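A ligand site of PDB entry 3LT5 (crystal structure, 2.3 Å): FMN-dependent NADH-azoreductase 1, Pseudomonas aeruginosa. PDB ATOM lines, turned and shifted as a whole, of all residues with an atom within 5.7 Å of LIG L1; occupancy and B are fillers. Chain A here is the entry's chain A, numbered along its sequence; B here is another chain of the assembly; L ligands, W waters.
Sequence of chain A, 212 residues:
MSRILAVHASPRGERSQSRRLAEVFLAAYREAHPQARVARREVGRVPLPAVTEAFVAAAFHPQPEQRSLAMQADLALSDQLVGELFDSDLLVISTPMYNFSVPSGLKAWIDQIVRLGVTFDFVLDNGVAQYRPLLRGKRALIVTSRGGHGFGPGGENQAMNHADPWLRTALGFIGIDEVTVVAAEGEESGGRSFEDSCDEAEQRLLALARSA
The side-chain amide nitrogen (ND2) of Asn 99 sits at hydrogen-bond distance from the side-chain carboxylate (OD1) of Asp 111 of chain B (2.7 Å). O of Gly 147 lies within hydrogen-bond range of N of Glu 187 (3.1 Å). The backbone NH (N) of Arg 12 sits at hydrogen-bond distance from the side-chain hydroxyl (OG) of Ser 10 (3.0 Å). The guanidinium group (NH2) of Arg 12 is in salt-bridge range of the side-chain carboxylate (OE2) of Glu 187 (3.2 Å). OG of Ser 18 lies within hydrogen-bond range of N of Thr 95. The backbone NH (N) of Glu 187 lies within hydrogen-bond range of the backbone carbonyl oxygen (O) of Arg 146 (3.0 Å). The side-chain hydroxyl of Ser 10 sits close to the side-chain hydroxyl of Ser 16 (3.4 Å). The side-chain hydroxyl (OG) of Ser 16 is in hydrogen-bond range of the backbone NH (N) of Arg 19 (2.9 Å).
An oxygen (O1) of LIG L1 is in hydrogen-bond range of the backbone NH (N) of Gly 148 (2.7 Å). The backbone NH (N) of Phe 100 lies within hydrogen-bond range of an oxygen (O2) of LIG L1, 2.9 Å away. The backbone carbonyl oxygen (O) of Met 97 sits at hydrogen-bond distance from an oxygen (O3) of LIG L1, 2.8 Å away. O9 of LIG L1 lies within hydrogen-bond range of N of Ser 18. OG of Ser 16 is in hydrogen-bond range of O9 of LIG L1 (2.7 Å). The side-chain carboxylate of Glu 187 sits at hydrogen-bond distance from an oxygen (O4) of LIG L1. The side-chain hydroxyl (OG) of Ser 18 lies within hydrogen-bond range of an oxygen (O9) of LIG L1. N3 of LIG L1 sits at hydrogen-bond distance from N of Asn 99. An oxygen (O8) of LIG L1 sits at hydrogen-bond distance from the side-chain hydroxyl (OG) of Ser 10, 2.7 Å away. A nitrogen (N1) of LIG L1 is in hydrogen-bond range of the backbone NH (N) of Gly 147, at 3.0 Å. A nitrogen (N2) of LIG L1 is in hydrogen-bond range of the side-chain sulfur (SD) of Met 97, at 3.5 Å. The backbone NH (N) of Gln 17 is in hydrogen-bond range of an oxygen (O7) of LIG L1 (2.8 Å). OG of Ser 145 lies within hydrogen-bond range of O5 of LIG L1 (2.8 Å). OE2 of Glu 188 sits close to O2 of LG2 L2. An oxygen (O7) of LIG L1 lies within salt-bridge range of the guanidinium group (NH2) of Arg 12 (2.7 Å). OD1 of Asn 99 sits close to O1 of LG2 L2, at 2.7 Å.
Water W2 lies within hydrogen-bond range of the side-chain hydroxyl of Tyr 98, an oxygen (O8) of LIG L1 and the guanidinium group of Arg 12. Water W3 bridges O of Asp 111 of chain B (2.7 Å) and ND2 of Asn 99 (3.2 Å).
Residues that only touch LIG L1: Pro 96 (3.2 Å), Glu 188 (3.3 Å), Tyr 98 (3.4 Å), Phe 151 (3.4 Å), Arg 146 (3.6 Å), Val 56 of chain B (3.7 Å), Phe 60 of chain B (3.7 Å) and Arg 15 (3.9 Å). Hydrophobic or aromatic side chains that line LIG L1: Pro 96, Met 97, Tyr 98, Phe 151, Val 56 of chain B and Phe 60 of chain B. Of the 29 residues printed, 20 come within 4 Å of LIG L1.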
ATOM      1  N   SER A  10      -6.949   7.330 -18.543  1.00  0.00           N
ATOM      2  CA  SER A  10      -6.000   8.137 -17.770  1.00  0.00           C
ATOM      3  C   SER A  10      -5.128   9.026 -18.677  1.00  0.00           C
ATOM      4  O   SER A  10      -4.666   8.567 -19.712  1.00  0.00           O
ATOM      5  CB  SER A  10      -5.115   7.259 -16.897  1.00  0.00           C
ATOM      6  OG  SER A  10      -4.112   8.030 -16.271  1.00  0.00           O
ATOM      7  N   PRO A  11      -4.902  10.291 -18.262  1.00  0.00           N
ATOM      8  CA  PRO A  11      -3.960  11.217 -18.914  1.00  0.00           C
ATOM      9  C   PRO A  11      -2.507  10.814 -18.675  1.00  0.00           C
ATOM     10  O   PRO A  11      -1.620  11.260 -19.385  1.00  0.00           O
ATOM     11  CB  PRO A  11      -4.213  12.557 -18.191  1.00  0.00           C
ATOM     12  CG  PRO A  11      -5.444  12.346 -17.392  1.00  0.00           C
ATOM     13  CD  PRO A  11      -5.538  10.899 -17.090  1.00  0.00           C
ATOM     14  N   ARG A  12      -2.271   9.992 -17.652  1.00  0.00           N
ATOM     15  CA  ARG A  12      -0.920   9.529 -17.357  1.00  0.00           C
ATOM     16  C   ARG A  12      -0.506   8.349 -18.231  1.00  0.00           C
ATOM     17  O   ARG A  12      -1.344   7.584 -18.705  1.00  0.00           O
ATOM     18  CB  ARG A  12      -0.780   9.201 -15.883  1.00  0.00           C
ATOM     19  CG  ARG A  12      -1.130  10.391 -14.981  1.00  0.00           C
ATOM     20  CD  ARG A  12      -0.498  10.226 -13.616  1.00  0.00           C
ATOM     21  NE  ARG A  12      -0.999   9.039 -12.927  1.00  0.00           N
ATOM     22  CZ  ARG A  12      -0.589   8.662 -11.717  1.00  0.00           C
ATOM     23  NH1 ARG A  12       0.335   9.388 -11.073  1.00  0.00           N
ATOM     24  NH2 ARG A  12      -1.100   7.582 -11.165  1.00  0.00           N
ATOM     25  N   ARG A  15       3.128   5.990 -15.703  1.00  0.00           N
ATOM     26  CA  ARG A  15       2.662   6.122 -14.323  1.00  0.00           C
ATOM     27  C   ARG A  15       1.187   5.766 -14.076  1.00  0.00           C
ATOM     28  O   ARG A  15       0.771   5.721 -12.931  1.00  0.00           O
ATOM     29  CB  ARG A  15       2.973   7.523 -13.772  1.00  0.00           C
ATOM     30  CG  ARG A  15       4.463   7.798 -13.656  1.00  0.00           C
ATOM     31  CD  ARG A  15       4.759   9.140 -13.016  1.00  0.00           C
ATOM     32  NE  ARG A  15       6.199   9.373 -12.950  1.00  0.00           N
ATOM     33  CZ  ARG A  15       6.855  10.201 -13.753  1.00  0.00           C
ATOM     34  NH1 ARG A  15       6.209  10.888 -14.682  1.00  0.00           N
ATOM     35  NH2 ARG A  15       8.170  10.343 -13.620  1.00  0.00           N
ATOM     36  N   SER A  16       0.393   5.547 -15.126  1.00  0.00           N
ATOM     37  CA  SER A  16      -1.009   5.223 -14.930  1.00  0.00           C
ATOM     38  C   SER A  16      -1.177   3.787 -14.407  1.00  0.00           C
ATOM     39  O   SER A  16      -0.718   2.832 -15.029  1.00  0.00           O
ATOM     40  CB  SER A  16      -1.815   5.395 -16.218  1.00  0.00           C
ATOM     41  OG  SER A  16      -3.087   4.773 -16.100  1.00  0.00           O
ATOM     42  N   GLN A  17      -1.833   3.646 -13.254  1.00  0.00           N
ATOM     43  CA  GLN A  17      -2.092   2.308 -12.716  1.00  0.00           C
ATOM     44  C   GLN A  17      -3.229   1.616 -13.472  1.00  0.00           C
ATOM     45  O   GLN A  17      -3.157   0.422 -13.738  1.00  0.00           O
ATOM     46  CB  GLN A  17      -2.391   2.353 -11.210  1.00  0.00           C
ATOM     47  CG  GLN A  17      -1.204   2.797 -10.382  1.00  0.00           C
ATOM     48  CD  GLN A  17      -0.011   1.824 -10.488  1.00  0.00           C
ATOM     49  OE1 GLN A  17      -0.152   0.653 -10.844  1.00  0.00           O
ATOM     50  NE2 GLN A  17       1.164   2.323 -10.151  1.00  0.00           N
ATOM     51  N   SER A  18      -4.276   2.363 -13.825  1.00  0.00           N
ATOM     52  CA  SER A  18      -5.384   1.763 -14.551  1.00  0.00           C
ATOM     53  C   SER A  18      -4.959   1.316 -15.967  1.00  0.00           C
ATOM     54  O   SER A  18      -5.373   0.258 -16.445  1.00  0.00           O
ATOM     55  CB  SER A  18      -6.614   2.682 -14.574  1.00  0.00           C
ATOM     56  OG  SER A  18      -6.415   3.804 -15.405  1.00  0.00           O
ATOM     57  N   ARG A  19      -4.112   2.107 -16.626  1.00  0.00           N
ATOM     58  CA  ARG A  19      -3.545   1.734 -17.911  1.00  0.00           C
ATOM     59  C   ARG A  19      -2.630   0.524 -17.751  1.00  0.00           C
ATOM     60  O   ARG A  19      -2.710  -0.447 -18.504  1.00  0.00           O
ATOM     61  CB  ARG A  19      -2.789   2.909 -18.521  1.00  0.00           C
ATOM     62  CG  ARG A  19      -2.175   2.652 -19.878  1.00  0.00           C
ATOM     63  CD  ARG A  19      -1.252   3.794 -20.307  1.00  0.00           C
ATOM     64  NE  ARG A  19      -1.964   5.078 -20.385  1.00  0.00           N
ATOM     65  CZ  ARG A  19      -2.672   5.488 -21.442  1.00  0.00           C
ATOM     66  NH1 ARG A  19      -2.786   4.712 -22.517  1.00  0.00           N
ATOM     67  NH2 ARG A  19      -3.280   6.677 -21.408  1.00  0.00           N
ATOM     68  N   THR A  95      -9.689   3.453 -16.400  1.00  0.00           N
ATOM     69  CA  THR A  95      -9.975   4.802 -15.944  1.00  0.00           C
ATOM     70  C   THR A  95      -9.607   5.041 -14.476  1.00  0.00           C
ATOM     71  O   THR A  95      -9.790   4.154 -13.633  1.00  0.00           O
ATOM     72  CB  THR A  95     -11.485   5.181 -16.169  1.00  0.00           C
ATOM     73  OG1 THR A  95     -11.716   6.502 -15.705  1.00  0.00           O
ATOM     74  CG2 THR A  95     -12.441   4.225 -15.422  1.00  0.00           C
ATOM     75  N   PRO A  96      -9.061   6.224 -14.180  1.00  0.00           N
ATOM     76  CA  PRO A  96      -8.962   6.722 -12.804  1.00  0.00           C
ATOM     77  C   PRO A  96     -10.346   7.035 -12.265  1.00  0.00           C
ATOM     78  O   PRO A  96     -11.296   7.142 -13.044  1.00  0.00           O
ATOM     79  CB  PRO A  96      -8.188   8.052 -12.951  1.00  0.00           C
ATOM     80  CG  PRO A  96      -7.653   8.063 -14.357  1.00  0.00           C
ATOM     81  CD  PRO A  96      -8.535   7.177 -15.171  1.00  0.00           C
ATOM     82  N   MET A  97     -10.472   7.176 -10.952  1.00  0.00           N
ATOM     83  CA  MET A  97     -11.581   7.934 -10.401  1.00  0.00           C
ATOM     84  C   MET A  97     -11.060   9.368 -10.288  1.00  0.00           C
ATOM     85  O   MET A  97     -10.015   9.602  -9.693  1.00  0.00           O
ATOM     86  CB  MET A  97     -12.003   7.413  -9.021  1.00  0.00           C
ATOM     87  CG  MET A  97     -12.982   8.342  -8.269  1.00  0.00           C
ATOM     88  SD  MET A  97     -13.707   7.684  -6.723  1.00  0.00           S
ATOM     89  CE  MET A  97     -15.033   6.666  -7.370  1.00  0.00           C
ATOM     90  N   TYR A  98     -11.754  10.315 -10.906  1.00  0.00           N
ATOM     91  CA  TYR A  98     -11.403  11.733 -10.737  1.00  0.00           C
ATOM     92  C   TYR A  98     -12.584  12.440 -10.148  1.00  0.00           C
ATOM     93  O   TYR A  98     -13.632  12.513 -10.779  1.00  0.00           O
ATOM     94  CB  TYR A  98     -11.106  12.406 -12.093  1.00  0.00           C
ATOM     95  CG  TYR A  98      -9.689  12.285 -12.591  1.00  0.00           C
ATOM     96  CD1 TYR A  98      -8.745  11.534 -11.914  1.00  0.00           C
ATOM     97  CD2 TYR A  98      -9.309  12.925 -13.770  1.00  0.00           C
ATOM     98  CE1 TYR A  98      -7.435  11.428 -12.386  1.00  0.00           C
ATOM     99  CE2 TYR A  98      -8.010  12.829 -14.255  1.00  0.00           C
ATOM    100  CZ  TYR A  98      -7.080  12.083 -13.548  1.00  0.00           C
ATOM    101  OH  TYR A  98      -5.781  12.004 -14.019  1.00  0.00           O
ATOM    102  N   ASN A  99     -12.423  12.979  -8.943  1.00  0.00           N
ATOM    103  CA  ASN A  99     -13.502  13.719  -8.295  1.00  0.00           C
ATOM    104  C   ASN A  99     -14.829  12.948  -8.287  1.00  0.00           C
ATOM    105  O   ASN A  99     -15.895  13.494  -8.638  1.00  0.00           O
ATOM    106  CB  ASN A  99     -13.647  15.106  -8.938  1.00  0.00           C
ATOM    107  CG  ASN A  99     -12.401  15.950  -8.747  1.00  0.00           C
ATOM    108  OD1 ASN A  99     -11.925  16.122  -7.631  1.00  0.00           O
ATOM    109  ND2 ASN A  99     -11.847  16.457  -9.856  1.00  0.00           N
ATOM    110  N   PHE A 100     -14.745  11.677  -7.896  1.00  0.00           N
ATOM    111  CA  PHE A 100     -15.927  10.842  -7.668  1.00  0.00           C
ATOM    112  C   PHE A 100     -16.562  10.372  -8.950  1.00  0.00           C
ATOM    113  O   PHE A 100     -17.549   9.635  -8.931  1.00  0.00           O
ATOM    114  CB  PHE A 100     -16.921  11.561  -6.744  1.00  0.00           C
ATOM    115  CG  PHE A 100     -16.292  12.006  -5.461  1.00  0.00           C
ATOM    116  CD1 PHE A 100     -15.916  11.068  -4.508  1.00  0.00           C
ATOM    117  CD2 PHE A 100     -16.032  13.355  -5.237  1.00  0.00           C
ATOM    118  CE1 PHE A 100     -15.306  11.474  -3.328  1.00  0.00           C
ATOM    119  CE2 PHE A 100     -15.428  13.766  -4.064  1.00  0.00           C
ATOM    120  CZ  PHE A 100     -15.060  12.821  -3.110  1.00  0.00           C
ATOM    121  N   SER A 101     -15.969  10.762 -10.074  1.00  0.00           N
ATOM    122  CA  SER A 101     -16.445  10.284 -11.359  1.00  0.00           C
ATOM    123  C   SER A 101     -15.270   9.875 -12.263  1.00  0.00           C
ATOM    124  O   SER A 101     -14.203   9.511 -11.774  1.00  0.00           O
ATOM    125  CB  SER A 101     -17.329  11.340 -12.023  1.00  0.00           C
ATOM    126  OG  SER A 101     -18.133  10.741 -13.019  1.00  0.00           O
ATOM    127  N   SER A 145      -8.648   2.582 -11.117  1.00  0.00           N
ATOM    128  CA  SER A 145      -7.738   2.876 -10.018  1.00  0.00           C
ATOM    129  C   SER A 145      -8.243   4.095  -9.235  1.00  0.00           C
ATOM    130  O   SER A 145      -8.718   5.060  -9.843  1.00  0.00           O
ATOM    131  CB  SER A 145      -6.311   3.122 -10.549  1.00  0.00           C
ATOM    132  OG  SER A 145      -5.408   3.258  -9.473  1.00  0.00           O
ATOM    133  N   ARG A 146      -8.144   4.040  -7.913  1.00  0.00           N
ATOM    134  CA  ARG A 146      -8.581   5.141  -7.049  1.00  0.00           C
ATOM    135  C   ARG A 146      -7.509   5.473  -6.012  1.00  0.00           C
ATOM    136  O   ARG A 146      -6.837   4.579  -5.485  1.00  0.00           O
ATOM    137  CB  ARG A 146      -9.872   4.764  -6.309  1.00  0.00           C
ATOM    138  CG  ARG A 146     -10.894   4.039  -7.155  1.00  0.00           C
ATOM    139  CD  ARG A 146     -12.147   3.674  -6.363  1.00  0.00           C
ATOM    140  NE  ARG A 146     -13.127   3.019  -7.223  1.00  0.00           N
ATOM    141  CZ  ARG A 146     -13.630   1.808  -7.003  1.00  0.00           C
ATOM    142  NH1 ARG A 146     -13.272   1.113  -5.927  1.00  0.00           N
ATOM    143  NH2 ARG A 146     -14.504   1.307  -7.851  1.00  0.00           N
ATOM    144  N   GLY A 147      -7.371   6.771  -5.709  1.00  0.00           N
ATOM    145  CA  GLY A 147      -6.468   7.226  -4.663  1.00  0.00           C
ATOM    146  C   GLY A 147      -6.900   6.810  -3.257  1.00  0.00           C
ATOM    147  O   GLY A 147      -6.070   6.378  -2.455  1.00  0.00           O
ATOM    148  N   GLY A 148      -8.202   6.937  -2.972  1.00  0.00           N
ATOM    149  CA  GLY A 148      -8.739   6.605  -1.656  1.00  0.00           C
ATOM    150  C   GLY A 148      -9.291   5.182  -1.524  1.00  0.00           C
ATOM    151  O   GLY A 148      -9.119   4.348  -2.416  1.00  0.00           O
ATOM    152  N   HIS A 149      -9.958   4.917  -0.395  1.00  0.00           N
ATOM    153  CA  HIS A 149     -10.483   3.581  -0.084  1.00  0.00           C
ATOM    154  C   HIS A 149     -11.979   3.630   0.155  1.00  0.00           C
ATOM    155  O   HIS A 149     -12.534   4.696   0.442  1.00  0.00           O
ATOM    156  CB  HIS A 149      -9.859   3.030   1.207  1.00  0.00           C
ATOM    157  CG  HIS A 149      -8.369   2.913   1.164  1.00  0.00           C
ATOM    158  ND1 HIS A 149      -7.732   1.769   0.748  1.00  0.00           N
ATOM    159  CD2 HIS A 149      -7.396   3.781   1.528  1.00  0.00           C
ATOM    160  CE1 HIS A 149      -6.421   1.939   0.845  1.00  0.00           C
ATOM    161  NE2 HIS A 149      -6.194   3.152   1.311  1.00  0.00           N
ATOM    162  N   PHE A 151     -14.713   2.813  -1.856  1.00  0.00           N
ATOM    163  CA  PHE A 151     -15.681   3.165  -2.903  1.00  0.00           C
ATOM    164  C   PHE A 151     -16.384   1.950  -3.543  1.00  0.00           C
ATOM    165  O   PHE A 151     -17.313   2.106  -4.333  1.00  0.00           O
ATOM    166  CB  PHE A 151     -15.030   4.028  -3.991  1.00  0.00           C
ATOM    167  CG  PHE A 151     -14.535   5.371  -3.488  1.00  0.00           C
ATOM    168  CD1 PHE A 151     -15.382   6.476  -3.467  1.00  0.00           C
ATOM    169  CD2 PHE A 151     -13.220   5.540  -3.078  1.00  0.00           C
ATOM    170  CE1 PHE A 151     -14.937   7.718  -3.012  1.00  0.00           C
ATOM    171  CE2 PHE A 151     -12.749   6.786  -2.612  1.00  0.00           C
ATOM    172  CZ  PHE A 151     -13.617   7.871  -2.574  1.00  0.00           C
ATOM    173  N   GLU A 187      -4.299   4.269  -3.932  1.00  0.00           N
ATOM    174  CA  GLU A 187      -3.163   4.712  -4.749  1.00  0.00           C
ATOM    175  C   GLU A 187      -2.453   5.927  -4.145  1.00  0.00           C
ATOM    176  O   GLU A 187      -1.223   6.037  -4.251  1.00  0.00           O
ATOM    177  CB  GLU A 187      -3.581   5.003  -6.198  1.00  0.00           C
ATOM    178  CG  GLU A 187      -2.420   5.079  -7.207  1.00  0.00           C
ATOM    179  CD  GLU A 187      -1.879   6.488  -7.415  1.00  0.00           C
ATOM    180  OE1 GLU A 187      -2.476   7.458  -6.892  1.00  0.00           O
ATOM    181  OE2 GLU A 187      -0.853   6.638  -8.119  1.00  0.00           O
ATOM    182  N   GLU A 188      -3.204   6.815  -3.510  1.00  0.00           N
ATOM    183  CA  GLU A 188      -2.625   8.058  -2.970  1.00  0.00           C
ATOM    184  C   GLU A 188      -1.849   7.801  -1.691  1.00  0.00           C
ATOM    185  O   GLU A 188      -0.966   8.587  -1.329  1.00  0.00           O
ATOM    186  CB  GLU A 188      -3.689   9.143  -2.768  1.00  0.00           C
ATOM    187  CG  GLU A 188      -3.991   9.923  -4.052  1.00  0.00           C
ATOM    188  CD  GLU A 188      -5.255  10.776  -3.977  1.00  0.00           C
ATOM    189  OE1 GLU A 188      -6.138  10.478  -3.143  1.00  0.00           O
ATOM    190  OE2 GLU A 188      -5.359  11.741  -4.777  1.00  0.00           O
ATOM    191  N   PHE A 194      -1.604  -0.829  -0.927  1.00  0.00           N
ATOM    192  CA  PHE A 194      -1.936  -0.549  -2.322  1.00  0.00           C
ATOM    193  C   PHE A 194      -1.291  -1.612  -3.211  1.00  0.00           C
ATOM    194  O   PHE A 194      -1.846  -1.997  -4.255  1.00  0.00           O
ATOM    195  CB  PHE A 194      -1.463   0.842  -2.743  1.00  0.00           C
ATOM    196  CG  PHE A 194      -1.706   1.150  -4.191  1.00  0.00           C
ATOM    197  CD1 PHE A 194      -2.996   1.251  -4.689  1.00  0.00           C
ATOM    198  CD2 PHE A 194      -0.642   1.338  -5.064  1.00  0.00           C
ATOM    199  CE1 PHE A 194      -3.221   1.529  -6.025  1.00  0.00           C
ATOM    200  CE2 PHE A 194      -0.860   1.622  -6.400  1.00  0.00           C
ATOM    201  CZ  PHE A 194      -2.150   1.712  -6.877  1.00  0.00           C
ATOM    202  N   VAL B  51      -8.035  17.666 -17.588  1.00  0.00           N
ATOM    203  CA  VAL B  51      -6.851  17.521 -16.764  1.00  0.00           C
ATOM    204  C   VAL B  51      -5.823  16.697 -17.553  1.00  0.00           C
ATOM    205  O   VAL B  51      -6.158  15.683 -18.155  1.00  0.00           O
ATOM    206  CB  VAL B  51      -7.194  16.853 -15.410  1.00  0.00           C
ATOM    207  CG1 VAL B  51      -6.006  16.104 -14.846  1.00  0.00           C
ATOM    208  CG2 VAL B  51      -7.724  17.880 -14.419  1.00  0.00           C
ATOM    209  N   PHE B  55      -0.864  18.859 -15.526  1.00  0.00           N
ATOM    210  CA  PHE B  55      -1.719  19.429 -14.499  1.00  0.00           C
ATOM    211  C   PHE B  55      -1.609  18.652 -13.187  1.00  0.00           C
ATOM    212  O   PHE B  55      -1.481  19.238 -12.100  1.00  0.00           O
ATOM    213  CB  PHE B  55      -3.156  19.481 -15.001  1.00  0.00           C
ATOM    214  CG  PHE B  55      -4.148  19.935 -13.963  1.00  0.00           C
ATOM    215  CD1 PHE B  55      -4.643  21.232 -13.973  1.00  0.00           C
ATOM    216  CD2 PHE B  55      -4.604  19.066 -12.982  1.00  0.00           C
ATOM    217  CE1 PHE B  55      -5.587  21.649 -13.032  1.00  0.00           C
ATOM    218  CE2 PHE B  55      -5.535  19.486 -12.035  1.00  0.00           C
ATOM    219  CZ  PHE B  55      -6.028  20.777 -12.067  1.00  0.00           C
ATOM    220  N   VAL B  56      -1.612  17.329 -13.276  1.00  0.00           N
ATOM    221  CA  VAL B  56      -1.502  16.492 -12.068  1.00  0.00           C
ATOM    222  C   VAL B  56      -0.165  16.773 -11.337  1.00  0.00           C
ATOM    223  O   VAL B  56      -0.132  16.923 -10.107  1.00  0.00           O
ATOM    224  CB  VAL B  56      -1.651  14.982 -12.385  1.00  0.00           C
ATOM    225  CG1 VAL B  56      -1.537  14.136 -11.114  1.00  0.00           C
ATOM    226  CG2 VAL B  56      -2.962  14.698 -13.141  1.00  0.00           C
ATOM    227  N   PHE B  60      -0.569  18.642  -7.573  1.00  0.00           N
ATOM    228  CA  PHE B  60      -0.121  17.844  -6.440  1.00  0.00           C
ATOM    229  C   PHE B  60       1.359  17.999  -6.120  1.00  0.00           C
ATOM    230  O   PHE B  60       1.914  17.185  -5.404  1.00  0.00           O
ATOM    231  CB  PHE B  60      -0.462  16.362  -6.665  1.00  0.00           C
ATOM    232  CG  PHE B  60      -1.935  16.096  -6.698  1.00  0.00           C
ATOM    233  CD1 PHE B  60      -2.620  15.782  -5.529  1.00  0.00           C
ATOM    234  CD2 PHE B  60      -2.652  16.217  -7.873  1.00  0.00           C
ATOM    235  CE1 PHE B  60      -3.991  15.570  -5.547  1.00  0.00           C
ATOM    236  CE2 PHE B  60      -4.021  15.988  -7.890  1.00  0.00           C
ATOM    237  CZ  PHE B  60      -4.689  15.671  -6.724  1.00  0.00           C
ATOM    238  N   ASP B 111     -13.086  19.354 -12.498  1.00  0.00           N
ATOM    239  CA  ASP B 111     -11.726  18.808 -12.394  1.00  0.00           C
ATOM    240  C   ASP B 111     -10.670  19.912 -12.224  1.00  0.00           C
ATOM    241  O   ASP B 111      -9.628  19.681 -11.616  1.00  0.00           O
ATOM    242  CB  ASP B 111     -11.396  17.892 -13.586  1.00  0.00           C
ATOM    243  CG  ASP B 111     -12.127  16.549 -13.515  1.00  0.00           C
ATOM    244  OD1 ASP B 111     -12.709  16.289 -12.438  1.00  0.00           O
ATOM    245  OD2 ASP B 111     -12.112  15.762 -14.526  1.00  0.00           O
HETATM  246  N1  LIG L   1      -8.996   9.313  -5.898  1.00  0.00           N
HETATM  247  C1  LIG L   1     -10.148   8.971  -5.218  1.00  0.00           C
HETATM  248  O1  LIG L   1     -10.197   7.985  -4.472  1.00  0.00           O
HETATM  249  N2  LIG L   1     -11.280   9.751  -5.369  1.00  0.00           N
HETATM  250  C2  LIG L   1     -11.277  10.864  -6.192  1.00  0.00           C
HETATM  251  O2  LIG L   1     -12.304  11.535  -6.316  1.00  0.00           O
HETATM  252  C3  LIG L   1     -10.105  11.214  -6.868  1.00  0.00           C
HETATM  253  N3  LIG L   1     -10.092  12.346  -7.685  1.00  0.00           N
HETATM  254  C4  LIG L   1      -8.924  12.673  -8.360  1.00  0.00           C
HETATM  255  C5  LIG L   1      -8.909  13.799  -9.199  1.00  0.00           C
HETATM  256  C6  LIG L   1      -7.752  14.135  -9.887  1.00  0.00           C
HETATM  257  C7  LIG L   1      -7.755  15.346 -10.783  1.00  0.00           C
HETATM  258  C8  LIG L   1      -6.595  13.342  -9.738  1.00  0.00           C
HETATM  259  C9  LIG L   1      -5.337  13.709 -10.488  1.00  0.00           C
HETATM  260  C10 LIG L   1      -6.616  12.221  -8.906  1.00  0.00           C
HETATM  261  C11 LIG L   1      -7.785  11.883  -8.223  1.00  0.00           C
HETATM  262  N4  LIG L   1      -7.808  10.779  -7.392  1.00  0.00           N
HETATM  263  C12 LIG L   1      -8.964  10.424  -6.717  1.00  0.00           C
HETATM  264  C13 LIG L   1      -6.576   9.919  -7.249  1.00  0.00           C
HETATM  265  C14 LIG L   1      -6.574   8.982  -8.468  1.00  0.00           C
HETATM  266  O3  LIG L   1      -7.812   8.315  -8.608  1.00  0.00           O
HETATM  267  C15 LIG L   1      -5.473   7.941  -8.412  1.00  0.00           C
HETATM  268  O4  LIG L   1      -4.223   8.615  -8.338  1.00  0.00           O
HETATM  269  C16 LIG L   1      -5.535   7.053  -9.661  1.00  0.00           C
HETATM  270  O5  LIG L   1      -4.702   5.932  -9.502  1.00  0.00           O
HETATM  271  C17 LIG L   1      -5.107   7.774 -10.940  1.00  0.00           C
HETATM  272  O6  LIG L   1      -5.308   6.911 -12.039  1.00  0.00           O
HETATM  273  P1  LIG L   1      -4.066   6.428 -12.948  1.00  0.00           P
HETATM  274  O7  LIG L   1      -3.007   5.825 -12.046  1.00  0.00           O
HETATM  275  O8  LIG L   1      -3.471   7.628 -13.676  1.00  0.00           O
HETATM  276  O9  LIG L   1      -4.537   5.396 -13.961  1.00  0.00           O
HETATM  277  C1  LG2 L   2     -10.160  11.520  -2.763  1.00  0.00           C
HETATM  278  C2  LG2 L   2     -11.636  11.944  -3.029  1.00  0.00           C
HETATM  279  C3  LG2 L   2     -11.931  13.016  -3.888  1.00  0.00           C
HETATM  280  C4  LG2 L   2     -10.807  13.763  -4.542  1.00  0.00           C
HETATM  281  C5  LG2 L   2      -9.364  13.358  -4.280  1.00  0.00           C
HETATM  282  C6  LG2 L   2      -9.058  12.275  -3.407  1.00  0.00           C
HETATM  283  C7  LG2 L   2     -12.059   9.034   0.804  1.00  0.00           C
HETATM  284  C8  LG2 L   2      -8.282  14.116  -4.950  1.00  0.00           C
HETATM  285  C9  LG2 L   2     -11.904  10.047  -0.282  1.00  0.00           C
HETATM  286  C10 LG2 L   2     -12.692  11.224  -0.241  1.00  0.00           C
HETATM  287  C11 LG2 L   2     -13.607  11.449   0.802  1.00  0.00           C
HETATM  288  C12 LG2 L   2     -13.757  10.420   1.917  1.00  0.00           C
HETATM  289  C13 LG2 L   2     -12.988   9.263   1.878  1.00  0.00           C
HETATM  290  N1  LG2 L   2     -10.965   9.830  -1.399  1.00  0.00           N
HETATM  291  N2  LG2 L   2      -9.883  10.652  -1.644  1.00  0.00           N
HETATM  292  O1  LG2 L   2     -11.082  14.827  -5.410  1.00  0.00           O
HETATM  293  O2  LG2 L   2      -6.963  13.783  -4.712  1.00  0.00           O
HETATM  294  O3  LG2 L   2      -8.608  15.168  -5.784  1.00  0.00           O
HETATM  295  O4  LG2 L   2     -14.922   9.753   4.082  1.00  0.00           O
HETATM  296  O   HOH W   1      -3.240  10.618 -10.279  1.00  0.00           O
HETATM  297  O   HOH W   2      -4.102  10.282 -12.792  1.00  0.00           O
HETATM  298  O   HOH W   3      -9.138  18.127  -9.519  1.00  0.00           O
